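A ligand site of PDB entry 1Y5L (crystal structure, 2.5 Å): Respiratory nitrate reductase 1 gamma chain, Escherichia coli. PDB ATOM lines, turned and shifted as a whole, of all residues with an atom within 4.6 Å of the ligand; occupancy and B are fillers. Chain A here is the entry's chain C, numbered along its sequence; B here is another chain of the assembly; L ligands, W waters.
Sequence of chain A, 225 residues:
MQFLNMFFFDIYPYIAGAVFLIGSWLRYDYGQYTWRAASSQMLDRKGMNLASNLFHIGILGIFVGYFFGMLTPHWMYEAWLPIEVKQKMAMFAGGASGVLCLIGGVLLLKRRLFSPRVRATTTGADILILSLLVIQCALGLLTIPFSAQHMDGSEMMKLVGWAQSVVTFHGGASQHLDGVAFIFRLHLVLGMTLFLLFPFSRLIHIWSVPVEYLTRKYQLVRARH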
ATOM      1  N   ALA A  37     -15.055   4.223 -32.977  1.00  0.00           N
ATOM      2  CA  ALA A  37     -16.245   3.965 -32.185  1.00  0.00           C
ATOM      3  C   ALA A  37     -17.454   4.694 -32.764  1.00  0.00           C
ATOM      4  O   ALA A  37     -18.597   4.349 -32.447  1.00  0.00           O
ATOM      5  CB  ALA A  37     -16.029   4.382 -30.750  1.00  0.00           C
ATOM      6  N   ALA A  38     -17.214   5.688 -33.604  1.00  0.00           N
ATOM      7  CA  ALA A  38     -18.299   6.448 -34.204  1.00  0.00           C
ATOM      8  C   ALA A  38     -19.177   7.102 -33.137  1.00  0.00           C
ATOM      9  O   ALA A  38     -20.401   6.989 -33.172  1.00  0.00           O
ATOM     10  CB  ALA A  38     -19.147   5.549 -35.104  1.00  0.00           C
ATOM     11  N   SER A  39     -18.557   7.784 -32.193  1.00  0.00           N
ATOM     12  CA  SER A  39     -19.317   8.449 -31.150  1.00  0.00           C
ATOM     13  C   SER A  39     -20.273   9.460 -31.783  1.00  0.00           C
ATOM     14  O   SER A  39     -19.943  10.094 -32.789  1.00  0.00           O
ATOM     15  CB  SER A  39     -18.402   9.181 -30.187  1.00  0.00           C
ATOM     16  OG  SER A  39     -19.163   9.969 -29.294  1.00  0.00           O
ATOM     17  N   SER A  40     -21.453   9.602 -31.181  1.00  0.00           N
ATOM     18  CA  SER A  40     -22.449  10.545 -31.687  1.00  0.00           C
ATOM     19  C   SER A  40     -22.860  11.435 -30.533  1.00  0.00           C
ATOM     20  O   SER A  40     -23.764  12.252 -30.659  1.00  0.00           O
ATOM     21  CB  SER A  40     -23.678   9.797 -32.216  1.00  0.00           C
ATOM     22  OG  SER A  40     -24.348   9.115 -31.170  1.00  0.00           O
ATOM     23  N   GLN A  41     -22.169  11.273 -29.409  1.00  0.00           N
ATOM     24  CA  GLN A  41     -22.453  12.035 -28.200  1.00  0.00           C
ATOM     25  C   GLN A  41     -22.469  13.555 -28.416  1.00  0.00           C
ATOM     26  O   GLN A  41     -23.426  14.228 -28.020  1.00  0.00           O
ATOM     27  CB  GLN A  41     -21.448  11.674 -27.108  1.00  0.00           C
ATOM     28  CG  GLN A  41     -21.738  12.292 -25.754  1.00  0.00           C
ATOM     29  CD  GLN A  41     -20.693  11.923 -24.708  1.00  0.00           C
ATOM     30  OE1 GLN A  41     -19.624  11.395 -25.028  1.00  0.00           O
ATOM     31  NE2 GLN A  41     -20.992  12.222 -23.447  1.00  0.00           N
ATOM     32  N   MET A  48     -27.498  10.375 -23.102  1.00  0.00           N
ATOM     33  CA  MET A  48     -26.427   9.468 -23.514  1.00  0.00           C
ATOM     34  C   MET A  48     -25.653   8.906 -22.330  1.00  0.00           C
ATOM     35  O   MET A  48     -25.246   7.735 -22.349  1.00  0.00           O
ATOM     36  CB  MET A  48     -25.449  10.165 -24.454  1.00  0.00           C
ATOM     37  CG  MET A  48     -25.805   9.985 -25.898  1.00  0.00           C
ATOM     38  SD  MET A  48     -25.937   8.241 -26.286  1.00  0.00           S
ATOM     39  CE  MET A  48     -24.339   7.933 -26.996  1.00  0.00           C
ATOM     40  N   SER A  52     -25.998   4.986 -22.636  1.00  0.00           N
ATOM     41  CA  SER A  52     -24.762   4.298 -22.992  1.00  0.00           C
ATOM     42  C   SER A  52     -24.167   3.482 -21.853  1.00  0.00           C
ATOM     43  O   SER A  52     -23.724   2.360 -22.066  1.00  0.00           O
ATOM     44  CB  SER A  52     -23.730   5.306 -23.504  1.00  0.00           C
ATOM     45  OG  SER A  52     -22.564   4.657 -23.975  1.00  0.00           O
ATOM     46  N   PHE A  55     -26.310   0.334 -21.201  1.00  0.00           N
ATOM     47  CA  PHE A  55     -26.045  -0.629 -22.248  1.00  0.00           C
ATOM     48  C   PHE A  55     -24.680  -1.297 -22.101  1.00  0.00           C
ATOM     49  O   PHE A  55     -24.590  -2.527 -22.052  1.00  0.00           O
ATOM     50  CB  PHE A  55     -26.171   0.029 -23.620  1.00  0.00           C
ATOM     51  CG  PHE A  55     -25.963  -0.904 -24.756  1.00  0.00           C
ATOM     52  CD1 PHE A  55     -24.764  -0.925 -25.451  1.00  0.00           C
ATOM     53  CD2 PHE A  55     -26.965  -1.802 -25.129  1.00  0.00           C
ATOM     54  CE1 PHE A  55     -24.555  -1.829 -26.491  1.00  0.00           C
ATOM     55  CE2 PHE A  55     -26.769  -2.711 -26.168  1.00  0.00           C
ATOM     56  CZ  PHE A  55     -25.558  -2.721 -26.844  1.00  0.00           C
ATOM     57  N   HIS A  56     -23.626  -0.495 -22.041  1.00  0.00           N
ATOM     58  CA  HIS A  56     -22.283  -1.063 -21.930  1.00  0.00           C
ATOM     59  C   HIS A  56     -22.042  -1.842 -20.644  1.00  0.00           C
ATOM     60  O   HIS A  56     -21.564  -2.982 -20.688  1.00  0.00           O
ATOM     61  CB  HIS A  56     -21.215   0.014 -22.134  1.00  0.00           C
ATOM     62  CG  HIS A  56     -21.003   0.396 -23.573  1.00  0.00           C
ATOM     63  ND1 HIS A  56     -21.661   1.437 -24.179  1.00  0.00           N
ATOM     64  CD2 HIS A  56     -20.262  -0.193 -24.547  1.00  0.00           C
ATOM     65  CE1 HIS A  56     -21.333   1.480 -25.460  1.00  0.00           C
ATOM     66  NE2 HIS A  56     -20.496   0.497 -25.707  1.00  0.00           N
ATOM     67  N   ILE A  59     -24.318  -5.115 -21.064  1.00  0.00           N
ATOM     68  CA  ILE A  59     -23.787  -6.092 -22.008  1.00  0.00           C
ATOM     69  C   ILE A  59     -22.413  -6.634 -21.586  1.00  0.00           C
ATOM     70  O   ILE A  59     -22.113  -7.813 -21.780  1.00  0.00           O
ATOM     71  CB  ILE A  59     -23.680  -5.519 -23.448  1.00  0.00           C
ATOM     72  CG1 ILE A  59     -23.468  -6.643 -24.465  1.00  0.00           C
ATOM     73  CG2 ILE A  59     -22.512  -4.555 -23.551  1.00  0.00           C
ATOM     74  CD1 ILE A  59     -24.688  -7.529 -24.659  1.00  0.00           C
ATOM     75  N   LEU A  60     -21.566  -5.780 -21.020  1.00  0.00           N
ATOM     76  CA  LEU A  60     -20.237  -6.236 -20.600  1.00  0.00           C
ATOM     77  C   LEU A  60     -20.312  -7.211 -19.433  1.00  0.00           C
ATOM     78  O   LEU A  60     -19.516  -8.140 -19.341  1.00  0.00           O
ATOM     79  CB  LEU A  60     -19.335  -5.051 -20.239  1.00  0.00           C
ATOM     80  CG  LEU A  60     -18.667  -4.330 -21.416  1.00  0.00           C
ATOM     81  CD1 LEU A  60     -17.854  -3.150 -20.902  1.00  0.00           C
ATOM     82  CD2 LEU A  60     -17.773  -5.286 -22.198  1.00  0.00           C
ATOM     83  N   PHE A  63     -21.191 -10.613 -20.844  1.00  0.00           N
ATOM     84  CA  PHE A  63     -20.052 -11.276 -21.471  1.00  0.00           C
ATOM     85  C   PHE A  63     -18.997 -11.786 -20.504  1.00  0.00           C
ATOM     86  O   PHE A  63     -18.346 -12.804 -20.755  1.00  0.00           O
ATOM     87  CB  PHE A  63     -19.398 -10.377 -22.530  1.00  0.00           C
ATOM     88  CG  PHE A  63     -20.035 -10.503 -23.890  1.00  0.00           C
ATOM     89  CD1 PHE A  63     -20.034 -11.718 -24.575  1.00  0.00           C
ATOM     90  CD2 PHE A  63     -20.696  -9.413 -24.449  1.00  0.00           C
ATOM     91  CE1 PHE A  63     -20.685 -11.847 -25.818  1.00  0.00           C
ATOM     92  CE2 PHE A  63     -21.357  -9.535 -25.685  1.00  0.00           C
ATOM     93  CZ  PHE A  63     -21.351 -10.763 -26.366  1.00  0.00           C
ATOM     94  N   LEU A 108     -30.921   3.892 -26.476  1.00  0.00           N
ATOM     95  CA  LEU A 108     -29.991   4.272 -27.523  1.00  0.00           C
ATOM     96  C   LEU A 108     -30.620   4.179 -28.914  1.00  0.00           C
ATOM     97  O   LEU A 108     -30.277   4.945 -29.806  1.00  0.00           O
ATOM     98  CB  LEU A 108     -28.751   3.377 -27.479  1.00  0.00           C
ATOM     99  CG  LEU A 108     -27.858   3.570 -26.247  1.00  0.00           C
ATOM    100  CD1 LEU A 108     -26.852   2.437 -26.163  1.00  0.00           C
ATOM    101  CD2 LEU A 108     -27.167   4.931 -26.337  1.00  0.00           C
ATOM    102  N   ARG A 111     -33.095   7.110 -29.501  1.00  0.00           N
ATOM    103  CA  ARG A 111     -32.315   8.308 -29.781  1.00  0.00           C
ATOM    104  C   ARG A 111     -31.814   8.284 -31.225  1.00  0.00           C
ATOM    105  O   ARG A 111     -31.913   9.278 -31.947  1.00  0.00           O
ATOM    106  CB  ARG A 111     -31.127   8.384 -28.813  1.00  0.00           C
ATOM    107  CG  ARG A 111     -30.100   9.473 -29.108  1.00  0.00           C
ATOM    108  CD  ARG A 111     -29.113   9.576 -27.965  1.00  0.00           C
ATOM    109  NE  ARG A 111     -27.951  10.400 -28.275  1.00  0.00           N
ATOM    110  CZ  ARG A 111     -27.017  10.073 -29.153  1.00  0.00           C
ATOM    111  NH1 ARG A 111     -25.995  10.895 -29.368  1.00  0.00           N
ATOM    112  NH2 ARG A 111     -27.097   8.940 -29.831  1.00  0.00           N
ATOM    113  N   ARG A 112     -31.281   7.140 -31.645  1.00  0.00           N
ATOM    114  CA  ARG A 112     -30.751   7.008 -32.997  1.00  0.00           C
ATOM    115  C   ARG A 112     -31.820   7.219 -34.043  1.00  0.00           C
ATOM    116  O   ARG A 112     -31.599   7.872 -35.065  1.00  0.00           O
ATOM    117  CB  ARG A 112     -30.077   5.641 -33.179  1.00  0.00           C
ATOM    118  CG  ARG A 112     -29.435   5.423 -34.544  1.00  0.00           C
ATOM    119  CD  ARG A 112     -28.388   4.315 -34.507  1.00  0.00           C
ATOM    120  NE  ARG A 112     -27.255   4.684 -33.655  1.00  0.00           N
ATOM    121  CZ  ARG A 112     -26.389   5.664 -33.938  1.00  0.00           C
ATOM    122  NH1 ARG A 112     -26.530   6.377 -35.044  1.00  0.00           N
ATOM    123  NH2 ARG A 112     -25.414   5.951 -33.092  1.00  0.00           N
ATOM    124  N   ILE A 129     -27.183  -3.050 -36.623  1.00  0.00           N
ATOM    125  CA  ILE A 129     -26.420  -3.677 -35.556  1.00  0.00           C
ATOM    126  C   ILE A 129     -27.006  -3.407 -34.161  1.00  0.00           C
ATOM    127  O   ILE A 129     -27.015  -4.295 -33.316  1.00  0.00           O
ATOM    128  CB  ILE A 129     -24.945  -3.250 -35.660  1.00  0.00           C
ATOM    129  CG1 ILE A 129     -24.048  -4.476 -35.478  1.00  0.00           C
ATOM    130  CG2 ILE A 129     -24.620  -2.190 -34.627  1.00  0.00           C
ATOM    131  CD1 ILE A 129     -24.051  -4.994 -34.080  1.00  0.00           C
ATOM    132  N   LEU A 130     -27.489  -2.190 -33.911  1.00  0.00           N
ATOM    133  CA  LEU A 130     -28.057  -1.868 -32.617  1.00  0.00           C
ATOM    134  C   LEU A 130     -29.436  -2.524 -32.427  1.00  0.00           C
ATOM    135  O   LEU A 130     -29.835  -2.858 -31.307  1.00  0.00           O
ATOM    136  CB  LEU A 130     -28.214  -0.359 -32.439  1.00  0.00           C
ATOM    137  CG  LEU A 130     -28.955   0.041 -31.166  1.00  0.00           C
ATOM    138  CD1 LEU A 130     -28.166  -0.427 -29.950  1.00  0.00           C
ATOM    139  CD2 LEU A 130     -29.159   1.549 -31.129  1.00  0.00           C
ATOM    140  N   LEU A 133     -28.928  -6.185 -31.559  1.00  0.00           N
ATOM    141  CA  LEU A 133     -28.431  -6.325 -30.194  1.00  0.00           C
ATOM    142  C   LEU A 133     -29.574  -6.176 -29.188  1.00  0.00           C
ATOM    143  O   LEU A 133     -29.591  -6.858 -28.160  1.00  0.00           O
ATOM    144  CB  LEU A 133     -27.349  -5.284 -29.906  1.00  0.00           C
ATOM    145  CG  LEU A 133     -25.957  -5.539 -30.472  1.00  0.00           C
ATOM    146  CD1 LEU A 133     -25.131  -4.258 -30.417  1.00  0.00           C
ATOM    147  CD2 LEU A 133     -25.265  -6.652 -29.690  1.00  0.00           C
ATOM    148  N   ARG A 202     -19.770  -1.096 -36.619  1.00  0.00           N
ATOM    149  CA  ARG A 202     -19.019  -0.351 -35.621  1.00  0.00           C
ATOM    150  C   ARG A 202     -18.499  -1.267 -34.508  1.00  0.00           C
ATOM    151  O   ARG A 202     -17.644  -0.868 -33.722  1.00  0.00           O
ATOM    152  CB  ARG A 202     -19.915   0.714 -35.004  1.00  0.00           C
ATOM    153  CG  ARG A 202     -21.088   0.148 -34.201  1.00  0.00           C
ATOM    154  CD  ARG A 202     -22.122   1.221 -33.896  1.00  0.00           C
ATOM    155  NE  ARG A 202     -21.521   2.360 -33.216  1.00  0.00           N
ATOM    156  CZ  ARG A 202     -22.089   3.559 -33.105  1.00  0.00           C
ATOM    157  NH1 ARG A 202     -23.285   3.778 -33.635  1.00  0.00           N
ATOM    158  NH2 ARG A 202     -21.450   4.533 -32.472  1.00  0.00           N
ATOM    159  N   LEU A 203     -19.000  -2.500 -34.435  1.00  0.00           N
ATOM    160  CA  LEU A 203     -18.575  -3.417 -33.382  1.00  0.00           C
ATOM    161  C   LEU A 203     -17.058  -3.588 -33.319  1.00  0.00           C
ATOM    162  O   LEU A 203     -16.528  -4.018 -32.298  1.00  0.00           O
ATOM    163  CB  LEU A 203     -19.239  -4.784 -33.532  1.00  0.00           C
ATOM    164  CG  LEU A 203     -20.764  -4.781 -33.380  1.00  0.00           C
ATOM    165  CD1 LEU A 203     -21.257  -6.212 -33.429  1.00  0.00           C
ATOM    166  CD2 LEU A 203     -21.165  -4.127 -32.059  1.00  0.00           C
ATOM    167  N   HIS A 205     -14.994  -1.639 -32.653  1.00  0.00           N
ATOM    168  CA  HIS A 205     -14.414  -0.859 -31.556  1.00  0.00           C
ATOM    169  C   HIS A 205     -14.096  -1.763 -30.389  1.00  0.00           C
ATOM    170  O   HIS A 205     -13.154  -1.501 -29.633  1.00  0.00           O
ATOM    171  CB  HIS A 205     -15.330   0.303 -31.090  1.00  0.00           C
ATOM    172  CG  HIS A 205     -16.580  -0.092 -30.352  1.00  0.00           C
ATOM    173  ND1 HIS A 205     -17.609  -0.780 -30.959  1.00  0.00           N
ATOM    174  CD2 HIS A 205     -17.023   0.218 -29.107  1.00  0.00           C
ATOM    175  CE1 HIS A 205     -18.634  -0.859 -30.129  1.00  0.00           C
ATOM    176  NE2 HIS A 205     -18.303  -0.268 -28.999  1.00  0.00           N
ATOM    177  N   ILE A 206     -14.857  -2.847 -30.263  1.00  0.00           N
ATOM    178  CA  ILE A 206     -14.634  -3.792 -29.176  1.00  0.00           C
ATOM    179  C   ILE A 206     -13.201  -4.336 -29.193  1.00  0.00           C
ATOM    180  O   ILE A 206     -12.608  -4.511 -28.137  1.00  0.00           O
ATOM    181  CB  ILE A 206     -15.629  -4.968 -29.230  1.00  0.00           C
ATOM    182  CG1 ILE A 206     -17.070  -4.438 -29.197  1.00  0.00           C
ATOM    183  CG2 ILE A 206     -15.426  -5.868 -28.022  1.00  0.00           C
ATOM    184  CD1 ILE A 206     -18.098  -5.474 -29.578  1.00  0.00           C
ATOM    185  N   VAL A 209     -10.494  -2.164 -27.137  1.00  0.00           N
ATOM    186  CA  VAL A 209     -10.594  -1.821 -25.715  1.00  0.00           C
ATOM    187  C   VAL A 209      -9.183  -1.466 -25.226  1.00  0.00           C
ATOM    188  O   VAL A 209      -8.295  -2.312 -25.176  1.00  0.00           O
ATOM    189  CB  VAL A 209     -11.228  -2.997 -24.909  1.00  0.00           C
ATOM    190  CG1 VAL A 209     -10.416  -4.273 -25.079  1.00  0.00           C
ATOM    191  CG2 VAL A 209     -11.369  -2.624 -23.447  1.00  0.00           C
ATOM    192  N   PRO A 210      -8.967  -0.178 -24.886  1.00  0.00           N
ATOM    193  CA  PRO A 210      -7.718   0.445 -24.408  1.00  0.00           C
ATOM    194  C   PRO A 210      -7.087  -0.019 -23.101  1.00  0.00           C
ATOM    195  O   PRO A 210      -6.833   0.793 -22.201  1.00  0.00           O
ATOM    196  CB  PRO A 210      -8.073   1.931 -24.356  1.00  0.00           C
ATOM    197  CG  PRO A 210      -9.495   1.880 -23.910  1.00  0.00           C
ATOM    198  CD  PRO A 210     -10.081   0.784 -24.794  1.00  0.00           C
ATOM    199  N   ILE B  88     -15.344   6.400 -20.371  1.00  0.00           N
ATOM    200  CA  ILE B  88     -15.299   6.061 -21.778  1.00  0.00           C
ATOM    201  C   ILE B  88     -16.640   5.788 -22.459  1.00  0.00           C
ATOM    202  O   ILE B  88     -16.819   6.075 -23.644  1.00  0.00           O
ATOM    203  CB  ILE B  88     -14.338   4.849 -21.978  1.00  0.00           C
ATOM    204  CG1 ILE B  88     -13.514   5.010 -23.256  1.00  0.00           C
ATOM    205  CG2 ILE B  88     -15.127   3.547 -21.939  1.00  0.00           C
ATOM    206  CD1 ILE B  88     -14.332   5.020 -24.498  1.00  0.00           C
ATOM    207  N   PHE B  89     -17.608   5.234 -21.737  1.00  0.00           N
ATOM    208  CA  PHE B  89     -18.891   4.938 -22.373  1.00  0.00           C
ATOM    209  C   PHE B  89     -19.657   6.196 -22.713  1.00  0.00           C
ATOM    210  O   PHE B  89     -20.434   6.223 -23.659  1.00  0.00           O
ATOM    211  CB  PHE B  89     -19.728   4.033 -21.476  1.00  0.00           C
ATOM    212  CG  PHE B  89     -19.068   2.730 -21.173  1.00  0.00           C
ATOM    213  CD1 PHE B  89     -18.451   2.008 -22.197  1.00  0.00           C
ATOM    214  CD2 PHE B  89     -19.040   2.233 -19.885  1.00  0.00           C
ATOM    215  CE1 PHE B  89     -17.816   0.795 -21.926  1.00  0.00           C
ATOM    216  CE2 PHE B  89     -18.401   1.012 -19.601  1.00  0.00           C
ATOM    217  CZ  PHE B  89     -17.794   0.296 -20.618  1.00  0.00           C
ATOM    218  N   TRP B 220     -12.326   7.703 -29.055  1.00  0.00           N
ATOM    219  CA  TRP B 220     -12.738   7.584 -27.660  1.00  0.00           C
ATOM    220  C   TRP B 220     -13.130   8.969 -27.141  1.00  0.00           C
ATOM    221  O   TRP B 220     -13.635   9.119 -26.027  1.00  0.00           O
ATOM    222  CB  TRP B 220     -11.575   7.037 -26.809  1.00  0.00           C
ATOM    223  CG  TRP B 220     -11.084   5.672 -27.198  1.00  0.00           C
ATOM    224  CD1 TRP B 220      -9.785   5.266 -27.317  1.00  0.00           C
ATOM    225  CD2 TRP B 220     -11.889   4.509 -27.463  1.00  0.00           C
ATOM    226  NE1 TRP B 220      -9.724   3.927 -27.626  1.00  0.00           N
ATOM    227  CE2 TRP B 220     -10.997   3.434 -27.716  1.00  0.00           C
ATOM    228  CE3 TRP B 220     -13.270   4.259 -27.497  1.00  0.00           C
ATOM    229  CZ2 TRP B 220     -11.450   2.146 -28.013  1.00  0.00           C
ATOM    230  CZ3 TRP B 220     -13.715   2.972 -27.783  1.00  0.00           C
ATOM    231  CH2 TRP B 220     -12.800   1.932 -28.035  1.00  0.00           C
ATOM    232  N   ARG B 221     -12.887   9.979 -27.966  1.00  0.00           N
ATOM    233  CA  ARG B 221     -13.193  11.373 -27.634  1.00  0.00           C
ATOM    234  C   ARG B 221     -13.008  11.809 -26.176  1.00  0.00           C
ATOM    235  O   ARG B 221     -13.869  12.465 -25.596  1.00  0.00           O
ATOM    236  CB  ARG B 221     -14.604  11.721 -28.110  1.00  0.00           C
ATOM    237  CG  ARG B 221     -15.682  10.712 -27.740  1.00  0.00           C
ATOM    238  CD  ARG B 221     -16.398  11.072 -26.451  1.00  0.00           C
ATOM    239  NE  ARG B 221     -17.500  10.157 -26.169  1.00  0.00           N
ATOM    240  CZ  ARG B 221     -17.363   8.963 -25.608  1.00  0.00           C
ATOM    241  NH1 ARG B 221     -16.164   8.532 -25.249  1.00  0.00           N
ATOM    242  NH2 ARG B 221     -18.430   8.191 -25.403  1.00  0.00           N
HETATM  243  C1  LIG L   1     -20.901   2.710 -28.869  1.00  0.00           C
HETATM  244  C2  LIG L   1     -16.908   2.200 -26.171  1.00  0.00           C
HETATM  245  C3  LIG L   1     -17.902  -2.540 -25.816  1.00  0.00           C
HETATM  246  C4  LIG L   1     -21.881  -2.027 -28.524  1.00  0.00           C
HETATM  247  C5  LIG L   1     -19.738   3.005 -28.180  1.00  0.00           C
HETATM  248  C6  LIG L   1     -19.094   4.310 -28.042  1.00  0.00           C
HETATM  249  C7  LIG L   1     -17.988   4.171 -27.304  1.00  0.00           C
HETATM  250  C8  LIG L   1     -17.914   2.751 -26.936  1.00  0.00           C
HETATM  251  C9  LIG L   1     -16.945   5.235 -26.847  1.00  0.00           C
HETATM  252  C10 LIG L   1     -19.628   5.614 -28.685  1.00  0.00           C
HETATM  253  C11 LIG L   1     -20.597   6.348 -27.664  1.00  0.00           C
HETATM  254  C12 LIG L   1     -21.010   7.768 -28.018  1.00  0.00           C
HETATM  255  O1  LIG L   1     -20.474   8.713 -27.363  1.00  0.00           O
HETATM  256  O2  LIG L   1     -21.865   7.888 -28.951  1.00  0.00           O
HETATM  257  C13 LIG L   1     -16.826   0.849 -25.827  1.00  0.00           C
HETATM  258  C14 LIG L   1     -15.750   0.247 -25.017  1.00  0.00           C
HETATM  259  C15 LIG L   1     -16.030  -1.084 -24.923  1.00  0.00           C
HETATM  260  C16 LIG L   1     -17.277  -1.317 -25.673  1.00  0.00           C
HETATM  261  C17 LIG L   1     -14.562   1.064 -24.431  1.00  0.00           C
HETATM  262  C18 LIG L   1     -15.217  -2.211 -24.168  1.00  0.00           C
HETATM  263  C19 LIG L   1     -14.996  -2.252 -22.819  1.00  0.00           C
HETATM  264  C20 LIG L   1     -19.056  -2.839 -26.503  1.00  0.00           C
HETATM  265  C21 LIG L   1     -19.690  -4.165 -26.623  1.00  0.00           C
HETATM  266  C22 LIG L   1     -20.799  -4.020 -27.384  1.00  0.00           C
HETATM  267  C23 LIG L   1     -20.884  -2.594 -27.744  1.00  0.00           C
HETATM  268  C24 LIG L   1     -19.116  -5.469 -25.965  1.00  0.00           C
HETATM  269  C25 LIG L   1     -21.862  -5.074 -27.836  1.00  0.00           C
HETATM  270  C26 LIG L   1     -21.513  -5.987 -28.786  1.00  0.00           C
HETATM  271  C27 LIG L   1     -21.962  -0.698 -28.861  1.00  0.00           C
HETATM  272  C28 LIG L   1     -23.046  -0.096 -29.682  1.00  0.00           C
HETATM  273  C29 LIG L   1     -22.761   1.226 -29.762  1.00  0.00           C
HETATM  274  C30 LIG L   1     -21.511   1.471 -29.005  1.00  0.00           C
HETATM  275  C31 LIG L   1     -24.246  -0.871 -30.295  1.00  0.00           C
HETATM  276  C32 LIG L   1     -23.525   2.425 -30.474  1.00  0.00           C
HETATM  277  C33 LIG L   1     -24.748   3.023 -29.661  1.00  0.00           C
HETATM  278  C34 LIG L   1     -25.674   3.935 -30.501  1.00  0.00           C
HETATM  279  O3  LIG L   1     -25.685   5.176 -30.186  1.00  0.00           O
HETATM  280  O4  LIG L   1     -26.350   3.349 -31.430  1.00  0.00           O
HETATM  281  N1  LIG L   1     -18.986   2.063 -27.493  1.00  0.00           N
HETATM  282  N2  LIG L   1     -17.733  -0.129 -26.217  1.00  0.00           N
HETATM  283  N3  LIG L   1     -19.804  -1.888 -27.193  1.00  0.00           N
HETATM  284  N4  LIG L   1     -21.061   0.295 -28.466  1.00  0.00           N
HETATM  285 FE1  LIG L   1     -19.400   0.116 -27.348  1.00  0.00          FE
HETATM  286  O   HOH W   1     -23.313   6.616 -30.825  1.00  0.00           O
HETATM  287  O   HOH W   2     -25.467   1.535 -33.106  1.00  0.00           O
HETATM  288  O   HOH W   3     -27.898   6.590 -30.026  1.00  0.00           O
HETATM  289  O   HOH W   4     -19.359   1.809 -31.407  1.00  0.00           O
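A ring nitrogen (NE2) of His 205 is bound to an iron atom (FE1) of the ligand (2.0 Å).
The backbone NH (N) of Ser 40 is in hydrogen-bond range of an oxygen (O2) of the ligand (2.8 Å).
FE1 of the ligand is bound by NE2 of His 56, at 2.0 Å.
An oxygen (O4) of the ligand lies within salt-bridge range of the guanidinium group of Arg 202 (3.8 Å).
The guanidinium group (NH2) of Arg 221 of chain B lies within salt-bridge range of an oxygen (O1) of the ligand (2.9 Å).
O1 of the ligand lies within hydrogen-bond range of OG of Ser 39.
The backbone NH (N) of Gln 41 lies within hydrogen-bond range of an oxygen (O2) of the ligand, at 3.4 Å.
The guanidinium group (NE) of Arg 112 is in salt-bridge range of an oxygen (O4) of the ligand.
The guanidinium group (NH2) of Arg 202 is in hydrogen-bond range of the backbone carbonyl oxygen (O) of Ala 37 (2.9 Å).
O of Phe 89 of chain B sits at hydrogen-bond distance from OG of Ser 52 (2.7 Å).
OG of Ser 39 sits at hydrogen-bond distance from N of Gln 41.
The guanidinium group (NE) of Arg 221 of chain B is in hydrogen-bond range of the side-chain amide oxygen (OE1) of Gln 41, 2.7 Å away.
ND1 of His 56 lies within hydrogen-bond range of O of Ser 52, at 3.1 Å.
The backbone carbonyl oxygen (O) of Ser 40 lies within hydrogen-bond range of the guanidinium group (NH1) of Arg 111 (2.9 Å).
The guanidinium group (NH2) of Arg 202 sits at hydrogen-bond distance from the backbone carbonyl oxygen (O) of Ala 38 (2.8 Å).
NH1 of Arg 221 of chain B is in hydrogen-bond range of O of Ile 88 of chain B, at 3.0 Å.
Merely in contact with the ligand: Ala 37 (3.97 Å), Met 48 (3.2 Å), Phe 55 (3.4 Å), Leu 60 (3.6 Å), Leu 130 (3.3 Å), Leu 133 (3.5 Å), Leu 203 (3.8 Å), Ile 206 (3.5 Å), Val 209 (3.7 Å), Ile 88 of chain B (3.3 Å), Phe 89 of chain B (3.8 Å) and Trp 220 of chain B (3.7 Å).
Of the 28 residues printed, 20 come within 4 Å of the ligand.
The nearest printed residue that does not touch the ligand is Arg 111 (4.04 Å).
Water W2 lies within hydrogen-bond range of an oxygen (O4) of the ligand (2.6 Å) and the guanidinium group (NH1) of Arg 202 (3.2 Å).
Water W3 lies within hydrogen-bond range of the guanidinium group of Arg 111 (2.5 Å), an oxygen (O3) of the ligand (2.6 Å) and the backbone carbonyl oxygen of Leu 108 (2.9 Å).
Water W1 lies within hydrogen-bond range of O2 of the ligand (2.7 Å), OG of Ser 40 (2.7 Å), NH2 of Arg 112 (3.2 Å) and NH2 of Arg 202 (3.2 Å).
Water W4 lies within hydrogen-bond range of the backbone carbonyl oxygen of Ala 37 (2.8 Å), the guanidinium group of Arg 202 (2.9 Å) and a ring nitrogen (ND1) of His 205 (3.2 Å).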
